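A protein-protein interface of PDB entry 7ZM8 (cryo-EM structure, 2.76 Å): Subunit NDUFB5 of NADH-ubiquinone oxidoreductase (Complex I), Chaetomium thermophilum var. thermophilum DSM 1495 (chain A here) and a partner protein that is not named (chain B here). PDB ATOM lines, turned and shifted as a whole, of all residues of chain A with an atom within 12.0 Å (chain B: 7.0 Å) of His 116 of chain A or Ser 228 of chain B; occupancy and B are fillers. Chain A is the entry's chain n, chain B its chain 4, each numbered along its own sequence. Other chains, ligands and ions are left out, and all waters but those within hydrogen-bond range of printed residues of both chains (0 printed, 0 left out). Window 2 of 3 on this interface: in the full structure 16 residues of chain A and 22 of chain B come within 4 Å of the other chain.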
ATOM      1  N   ALA A 107      -0.087   0.142   6.563  1.00  0.00           N
ATOM      2  CA  ALA A 107      -0.235   0.715   7.919  1.00  0.00           C
ATOM      3  C   ALA A 107      -1.371   1.726   7.956  1.00  0.00           C
ATOM      4  O   ALA A 107      -2.174   1.683   8.885  1.00  0.00           O
ATOM      5  CB  ALA A 107       1.053   1.365   8.308  1.00  0.00           C
ATOM      6  N   LEU A 108      -1.402   2.635   6.986  1.00  0.00           N
ATOM      7  CA  LEU A 108      -2.443   3.692   6.959  1.00  0.00           C
ATOM      8  C   LEU A 108      -3.798   3.038   6.718  1.00  0.00           C
ATOM      9  O   LEU A 108      -4.805   3.631   7.135  1.00  0.00           O
ATOM     10  CB  LEU A 108      -2.058   4.746   5.921  1.00  0.00           C
ATOM     11  CG  LEU A 108      -1.043   5.761   6.441  1.00  0.00           C
ATOM     12  CD1 LEU A 108      -0.086   6.208   5.355  1.00  0.00           C
ATOM     13  CD2 LEU A 108      -1.742   6.947   7.079  1.00  0.00           C
ATOM     14  N   GLU A 109      -3.823   1.867   6.080  1.00  0.00           N
ATOM     15  CA  GLU A 109      -5.083   1.099   5.962  1.00  0.00           C
ATOM     16  C   GLU A 109      -5.448   0.518   7.327  1.00  0.00           C
ATOM     17  O   GLU A 109      -6.653   0.497   7.642  1.00  0.00           O
ATOM     18  CB  GLU A 109      -4.890  -0.066   5.005  1.00  0.00           C
ATOM     19  CG  GLU A 109      -5.010   0.306   3.541  1.00  0.00           C
ATOM     20  CD  GLU A 109      -6.436   0.408   3.032  1.00  0.00           C
ATOM     21  OE1 GLU A 109      -7.361   0.090   3.804  1.00  0.00           O
ATOM     22  OE2 GLU A 109      -6.617   0.806   1.867  1.00  0.00           O
ATOM     23  N   GLN A 110      -4.477   0.052   8.104  1.00  0.00           N
ATOM     24  CA  GLN A 110      -4.758  -0.495   9.454  1.00  0.00           C
ATOM     25  C   GLN A 110      -5.315   0.617  10.338  1.00  0.00           C
ATOM     26  O   GLN A 110      -6.301   0.374  11.035  1.00  0.00           O
ATOM     27  CB  GLN A 110      -3.519  -1.123  10.079  1.00  0.00           C
ATOM     28  CG  GLN A 110      -3.766  -1.732  11.451  1.00  0.00           C
ATOM     29  CD  GLN A 110      -4.734  -2.889  11.407  1.00  0.00           C
ATOM     30  OE1 GLN A 110      -5.618  -3.018  12.250  1.00  0.00           O
ATOM     31  NE2 GLN A 110      -4.576  -3.743  10.409  1.00  0.00           N
ATOM     32  N   ALA A 111      -4.669   1.777  10.348  1.00  0.00           N
ATOM     33  CA  ALA A 111      -5.071   2.893  11.219  1.00  0.00           C
ATOM     34  C   ALA A 111      -6.492   3.343  10.899  1.00  0.00           C
ATOM     35  O   ALA A 111      -7.166   3.798  11.824  1.00  0.00           O
ATOM     36  CB  ALA A 111      -4.070   3.993  11.050  1.00  0.00           C
ATOM     37  N   ALA A 112      -6.906   3.292   9.638  1.00  0.00           N
ATOM     38  CA  ALA A 112      -8.299   3.625   9.262  1.00  0.00           C
ATOM     39  C   ALA A 112      -9.282   2.667   9.945  1.00  0.00           C
ATOM     40  O   ALA A 112     -10.333   3.134  10.379  1.00  0.00           O
ATOM     41  CB  ALA A 112      -8.416   3.503   7.772  1.00  0.00           C
ATOM     42  N   HIS A 113      -8.958   1.376   9.994  1.00  0.00           N
ATOM     43  CA  HIS A 113      -9.797   0.354  10.654  1.00  0.00           C
ATOM     44  C   HIS A 113      -9.822   0.689  12.137  1.00  0.00           C
ATOM     45  O   HIS A 113     -10.902   0.593  12.743  1.00  0.00           O
ATOM     46  CB  HIS A 113      -9.153  -1.014  10.405  1.00  0.00           C
ATOM     47  CG  HIS A 113      -9.804  -2.174  11.071  1.00  0.00           C
ATOM     48  ND1 HIS A 113     -10.440  -3.157  10.350  1.00  0.00           N
ATOM     49  CD2 HIS A 113      -9.876  -2.542  12.367  1.00  0.00           C
ATOM     50  CE1 HIS A 113     -10.896  -4.076  11.173  1.00  0.00           C
ATOM     51  NE2 HIS A 113     -10.565  -3.719  12.419  1.00  0.00           N
ATOM     52  N   ASP A 114      -8.674   1.074  12.690  1.00  0.00           N
ATOM     53  CA  ASP A 114      -8.560   1.384  14.140  1.00  0.00           C
ATOM     54  C   ASP A 114      -9.372   2.636  14.462  1.00  0.00           C
ATOM     55  O   ASP A 114     -10.054   2.620  15.486  1.00  0.00           O
ATOM     56  CB  ASP A 114      -7.101   1.407  14.583  1.00  0.00           C
ATOM     57  CG  ASP A 114      -6.446   0.044  14.487  1.00  0.00           C
ATOM     58  OD1 ASP A 114      -7.153  -0.912  14.122  1.00  0.00           O
ATOM     59  OD2 ASP A 114      -5.240  -0.049  14.783  1.00  0.00           O
ATOM     60  N   LYS A 115      -9.240   3.685  13.653  1.00  0.00           N
ATOM     61  CA  LYS A 115      -9.962   4.963  13.877  1.00  0.00           C
ATOM     62  C   LYS A 115     -11.453   4.680  13.871  1.00  0.00           C
ATOM     63  O   LYS A 115     -12.161   5.295  14.667  1.00  0.00           O
ATOM     64  CB  LYS A 115      -9.621   5.979  12.785  1.00  0.00           C
ATOM     65  CG  LYS A 115     -10.547   7.181  12.666  1.00  0.00           C
ATOM     66  CD  LYS A 115     -10.170   8.105  11.532  1.00  0.00           C
ATOM     67  CE  LYS A 115     -11.263   9.086  11.164  1.00  0.00           C
ATOM     68  NZ  LYS A 115     -10.872   9.930  10.011  1.00  0.00           N
ATOM     69  N   HIS A 116     -11.887   3.719  13.060  1.00  0.00           N
ATOM     70  CA  HIS A 116     -13.324   3.391  12.951  1.00  0.00           C
ATOM     71  C   HIS A 116     -13.710   2.596  14.199  1.00  0.00           C
ATOM     72  O   HIS A 116     -14.773   2.838  14.722  1.00  0.00           O
ATOM     73  CB  HIS A 116     -13.555   2.567  11.681  1.00  0.00           C
ATOM     74  CG  HIS A 116     -13.898   3.358  10.466  1.00  0.00           C
ATOM     75  ND1 HIS A 116     -14.160   2.755   9.255  1.00  0.00           N
ATOM     76  CD2 HIS A 116     -14.035   4.684  10.265  1.00  0.00           C
ATOM     77  CE1 HIS A 116     -14.441   3.674   8.359  1.00  0.00           C
ATOM     78  NE2 HIS A 116     -14.372   4.861   8.953  1.00  0.00           N
ATOM     79  N   LEU A 117     -12.829   1.717  14.679  1.00  0.00           N
ATOM     80  CA  LEU A 117     -13.153   0.881  15.868  1.00  0.00           C
ATOM     81  C   LEU A 117     -13.279   1.746  17.123  1.00  0.00           C
ATOM     82  O   LEU A 117     -14.247   1.575  17.857  1.00  0.00           O
ATOM     83  CB  LEU A 117     -12.046  -0.165  16.025  1.00  0.00           C
ATOM     84  CG  LEU A 117     -12.221  -1.169  17.160  1.00  0.00           C
ATOM     85  CD1 LEU A 117     -13.290  -2.192  16.811  1.00  0.00           C
ATOM     86  CD2 LEU A 117     -10.903  -1.855  17.464  1.00  0.00           C
ATOM     87  N   LEU A 118     -12.345   2.671  17.329  1.00  0.00           N
ATOM     88  CA  LEU A 118     -12.349   3.515  18.547  1.00  0.00           C
ATOM     89  C   LEU A 118     -13.468   4.557  18.485  1.00  0.00           C
ATOM     90  O   LEU A 118     -14.036   4.852  19.543  1.00  0.00           O
ATOM     91  CB  LEU A 118     -10.980   4.185  18.676  1.00  0.00           C
ATOM     92  CG  LEU A 118      -9.817   3.282  19.077  1.00  0.00           C
ATOM     93  CD1 LEU A 118      -8.493   3.918  18.683  1.00  0.00           C
ATOM     94  CD2 LEU A 118      -9.842   2.994  20.567  1.00  0.00           C
ATOM     95  N   LEU A 119     -13.785   5.077  17.300  1.00  0.00           N
ATOM     96  CA  LEU A 119     -14.774   6.184  17.187  1.00  0.00           C
ATOM     97  C   LEU A 119     -16.212   5.667  17.089  1.00  0.00           C
ATOM     98  O   LEU A 119     -17.125   6.503  17.167  1.00  0.00           O
ATOM     99  CB  LEU A 119     -14.411   7.030  15.963  1.00  0.00           C
ATOM    100  CG  LEU A 119     -14.200   8.522  16.199  1.00  0.00           C
ATOM    101  CD1 LEU A 119     -13.285   8.759  17.386  1.00  0.00           C
ATOM    102  CD2 LEU A 119     -13.629   9.174  14.953  1.00  0.00           C
ATOM    103  N   THR A 120     -16.413   4.365  16.890  1.00  0.00           N
ATOM    104  CA  THR A 120     -17.790   3.839  16.694  1.00  0.00           C
ATOM    105  C   THR A 120     -18.056   2.794  17.766  1.00  0.00           C
ATOM    106  O   THR A 120     -18.698   1.781  17.445  1.00  0.00           O
ATOM    107  CB  THR A 120     -18.012   3.223  15.304  1.00  0.00           C
ATOM    108  OG1 THR A 120     -17.191   2.066  15.163  1.00  0.00           O
ATOM    109  CG2 THR A 120     -17.769   4.186  14.165  1.00  0.00           C
ATOM    110  N   ALA A 121     -17.632   3.063  18.998  1.00  0.00           N
ATOM    111  CA  ALA A 121     -17.740   2.039  20.043  1.00  0.00           C
ATOM    112  C   ALA A 121     -19.028   2.203  20.840  1.00  0.00           C
ATOM    113  O   ALA A 121     -19.566   3.305  20.865  1.00  0.00           O
ATOM    114  CB  ALA A 121     -16.489   2.055  20.881  1.00  0.00           C
ATOM    115  N   GLU A 122     -19.514   1.110  21.424  1.00  0.00           N
ATOM    116  CA  GLU A 122     -20.791   1.155  22.165  1.00  0.00           C
ATOM    117  C   GLU A 122     -20.649   2.085  23.372  1.00  0.00           C
ATOM    118  O   GLU A 122     -19.680   1.954  24.108  1.00  0.00           O
ATOM    119  CB  GLU A 122     -21.187  -0.264  22.570  1.00  0.00           C
ATOM    120  CG  GLU A 122     -22.535  -0.355  23.260  1.00  0.00           C
ATOM    121  CD  GLU A 122     -23.741  -0.136  22.362  1.00  0.00           C
ATOM    122  OE1 GLU A 122     -23.588  -0.243  21.128  1.00  0.00           O
ATOM    123  OE2 GLU A 122     -24.832   0.139  22.898  1.00  0.00           O
ATOM    124  N   ARG A 123     -21.603   2.987  23.552  1.00  0.00           N
ATOM    125  CA  ARG A 123     -21.604   3.886  24.724  1.00  0.00           C
ATOM    126  C   ARG A 123     -22.178   3.064  25.865  1.00  0.00           C
ATOM    127  O   ARG A 123     -23.069   2.248  25.603  1.00  0.00           O
ATOM    128  CB  ARG A 123     -22.534   5.071  24.435  1.00  0.00           C
ATOM    129  CG  ARG A 123     -22.551   6.176  25.475  1.00  0.00           C
ATOM    130  CD  ARG A 123     -23.742   7.067  25.186  1.00  0.00           C
ATOM    131  NE  ARG A 123     -23.653   8.355  25.852  1.00  0.00           N
ATOM    132  CZ  ARG A 123     -23.373   9.493  25.237  1.00  0.00           C
ATOM    133  NH1 ARG A 123     -23.178   9.508  23.931  1.00  0.00           N
ATOM    134  NH2 ARG A 123     -23.306  10.614  25.926  1.00  0.00           N
ATOM    135  N   ILE B 223     -13.921  17.093   2.469  1.00  0.00           N
ATOM    136  CA  ILE B 223     -12.723  16.280   2.813  1.00  0.00           C
ATOM    137  C   ILE B 223     -12.981  15.540   4.119  1.00  0.00           C
ATOM    138  O   ILE B 223     -12.641  14.370   4.187  1.00  0.00           O
ATOM    139  CB  ILE B 223     -11.495  17.209   2.897  1.00  0.00           C
ATOM    140  CG1 ILE B 223     -11.035  17.681   1.517  1.00  0.00           C
ATOM    141  CG2 ILE B 223     -10.356  16.578   3.681  1.00  0.00           C
ATOM    142  CD1 ILE B 223      -9.892  18.660   1.566  1.00  0.00           C
ATOM    143  N   LEU B 224     -13.595  16.211   5.088  1.00  0.00           N
ATOM    144  CA  LEU B 224     -13.849  15.623   6.413  1.00  0.00           C
ATOM    145  C   LEU B 224     -14.813  14.464   6.271  1.00  0.00           C
ATOM    146  O   LEU B 224     -14.642  13.477   6.976  1.00  0.00           O
ATOM    147  CB  LEU B 224     -14.346  16.713   7.365  1.00  0.00           C
ATOM    148  CG  LEU B 224     -13.298  17.738   7.795  1.00  0.00           C
ATOM    149  CD1 LEU B 224     -13.880  18.743   8.776  1.00  0.00           C
ATOM    150  CD2 LEU B 224     -12.070  17.059   8.371  1.00  0.00           C
ATOM    151  N   THR B 225     -15.792  14.601   5.400  1.00  0.00           N
ATOM    152  CA  THR B 225     -16.758  13.511   5.137  1.00  0.00           C
ATOM    153  C   THR B 225     -16.061  12.279   4.549  1.00  0.00           C
ATOM    154  O   THR B 225     -16.310  11.189   5.031  1.00  0.00           O
ATOM    155  CB  THR B 225     -17.857  14.044   4.216  1.00  0.00           C
ATOM    156  OG1 THR B 225     -18.489  15.111   4.920  1.00  0.00           O
ATOM    157  CG2 THR B 225     -18.869  12.988   3.830  1.00  0.00           C
ATOM    158  N   MET B 226     -15.180  12.459   3.576  1.00  0.00           N
ATOM    159  CA  MET B 226     -14.479  11.316   2.956  1.00  0.00           C
ATOM    160  C   MET B 226     -13.604  10.621   3.997  1.00  0.00           C
ATOM    161  O   MET B 226     -13.543   9.395   3.967  1.00  0.00           O
ATOM    162  CB  MET B 226     -13.574  11.769   1.812  1.00  0.00           C
ATOM    163  CG  MET B 226     -14.272  12.481   0.709  1.00  0.00           C
ATOM    164  SD  MET B 226     -13.032  13.002  -0.475  1.00  0.00           S
ATOM    165  CE  MET B 226     -14.030  14.052  -1.527  1.00  0.00           C
ATOM    166  N   SER B 227     -12.943  11.384   4.865  1.00  0.00           N
ATOM    167  CA  SER B 227     -12.061  10.820   5.909  1.00  0.00           C
ATOM    168  C   SER B 227     -12.902  10.024   6.895  1.00  0.00           C
ATOM    169  O   SER B 227     -12.426   9.004   7.368  1.00  0.00           O
ATOM    170  CB  SER B 227     -11.349  11.922   6.592  1.00  0.00           C
ATOM    171  OG  SER B 227     -10.375  11.414   7.490  1.00  0.00           O
ATOM    172  N   SER B 228     -14.102  10.501   7.197  1.00  0.00           N
ATOM    173  CA  SER B 228     -15.013   9.809   8.137  1.00  0.00           C
ATOM    174  C   SER B 228     -15.438   8.472   7.556  1.00  0.00           C
ATOM    175  O   SER B 228     -15.468   7.510   8.305  1.00  0.00           O
ATOM    176  CB  SER B 228     -16.192  10.665   8.480  1.00  0.00           C
ATOM    177  OG  SER B 228     -17.162  10.637   7.450  1.00  0.00           O
ATOM    178  N   ILE B 229     -15.679   8.415   6.254  1.00  0.00           N
ATOM    179  CA  ILE B 229     -16.205   7.188   5.599  1.00  0.00           C
ATOM    180  C   ILE B 229     -15.062   6.206   5.351  1.00  0.00           C
ATOM    181  O   ILE B 229     -15.303   5.007   5.434  1.00  0.00           O
ATOM    182  CB  ILE B 229     -16.907   7.600   4.290  1.00  0.00           C
ATOM    183  CG1 ILE B 229     -18.074   8.552   4.552  1.00  0.00           C
ATOM    184  CG2 ILE B 229     -17.345   6.388   3.479  1.00  0.00           C
ATOM    185  CD1 ILE B 229     -18.776   9.018   3.307  1.00  0.00           C
ATOM    186  N   VAL B 230     -13.861   6.695   5.096  1.00  0.00           N
ATOM    187  CA  VAL B 230     -12.725   5.793   4.747  1.00  0.00           C
ATOM    188  C   VAL B 230     -11.737   5.608   5.912  1.00  0.00           C
ATOM    189  O   VAL B 230     -11.155   4.529   6.010  1.00  0.00           O
ATOM    190  CB  VAL B 230     -12.039   6.307   3.463  1.00  0.00           C
ATOM    191  CG1 VAL B 230     -10.828   5.481   3.063  1.00  0.00           C
ATOM    192  CG2 VAL B 230     -13.010   6.411   2.303  1.00  0.00           C
ATOM    193  N   GLY B 231     -11.567   6.605   6.774  1.00  0.00           N
ATOM    194  CA  GLY B 231     -10.684   6.493   7.946  1.00  0.00           C
ATOM    195  C   GLY B 231      -9.334   7.136   7.737  1.00  0.00           C
ATOM    196  O   GLY B 231      -8.564   7.211   8.695  1.00  0.00           O
ATOM    197  N   THR B 232      -9.060   7.588   6.521  1.00  0.00           N
ATOM    198  CA  THR B 232      -7.782   8.284   6.272  1.00  0.00           C
ATOM    199  C   THR B 232      -7.913   9.039   4.957  1.00  0.00           C
ATOM    200  O   THR B 232      -8.891   8.795   4.248  1.00  0.00           O
ATOM    201  CB  THR B 232      -6.606   7.297   6.163  1.00  0.00           C
ATOM    202  OG1 THR B 232      -5.410   8.002   5.837  1.00  0.00           O
ATOM    203  CG2 THR B 232      -6.831   6.210   5.137  1.00  0.00           C
ATOM    204  N   THR B 233      -7.030  10.009   4.733  1.00  0.00           N
ATOM    205  CA  THR B 233      -7.022  10.792   3.471  1.00  0.00           C
ATOM    206  C   THR B 233      -5.754  10.493   2.676  1.00  0.00           C
ATOM    207  O   THR B 233      -5.533  11.207   1.695  1.00  0.00           O
ATOM    208  CB  THR B 233      -7.230  12.282   3.769  1.00  0.00           C
ATOM    209  OG1 THR B 233      -6.314  12.689   4.784  1.00  0.00           O
ATOM    210  CG2 THR B 233      -8.639  12.589   4.214  1.00  0.00           C
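Of the 11 printed residues of chain B, 6 touch a printed residue of chain A. Along chain B the printed residues that touch a printed residue of chain A span positions 227 to 232. Among the printed residues, 8 pairs touch across the chains. Among the printed residues, no Asp or Glu carboxylate lies within 4 Å of a Lys or Arg side-chain nitrogen of the other chain.
His 116 of chain A touches just these residues of chain B: Ser 228, Ile 229 and Gly 231. Ser 228 of chain B touches just one residue of chain A: His 116. No residue of chain A comes within 4 Å of Thr 225 of chain B. Of chain A, only Lys 115 comes within 4 Å of Ser 227 of chain B. Val 230 of chain B touches just one residue of chain A: Ala 112. Printed residues of chain B within 4 Å of Ala 112 of chain A: Val 230 and Gly 231. Printed residues of chain B within 4 Å of Lys 115 of chain A: Ser 227 and Gly 231. Of the printed residues of chain B, Leu 108 of chain A touches Thr 232 (3.8 Å). Asp 114 of chain A touches none of the printed residues of chain B. The nearest residue of chain A that does not touch Ser 228 of chain B is Lys 115 of chain A (4.3 Å). The nearest printed residue of chain B that does not touch Leu 108 of chain A is Gly 231 of chain B (5.4 Å).
O of Leu 108 of chain A touches CG2 of Thr 232 of chain B (3.8 Å). Ala 112 of chain A touches Val 230 of chain B (CB to O, 3.4 Å). Gly 231 of chain B touches Ala 112 of chain A (O to CA, 3.6 Å). Lys 115 of chain A touches Gly 231 of chain B (CD to O, 3.4 Å). Ile 229 of chain B touches His 116 of chain A (O to CE1, 3.3 Å). His 116 of chain A touches Gly 231 of chain B.
The side-chain hydroxyl of Ser 227 of chain B is in hydrogen-bond range of the side-chain amino group of Lys 115 of chain A. A ring nitrogen (NE2) of His 116 of chain A lies within hydrogen-bond range of the backbone carbonyl oxygen (O) of Ser 228 of chain B, at 2.9 Å.
O of Thr 225 of chain B sits at hydrogen-bond distance from OG of Ser 228 of chain B, 2.6 Å away. O of His 116 of chain A sits at hydrogen-bond distance from OG1 of Thr 120 of chain A (2.6 Å).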
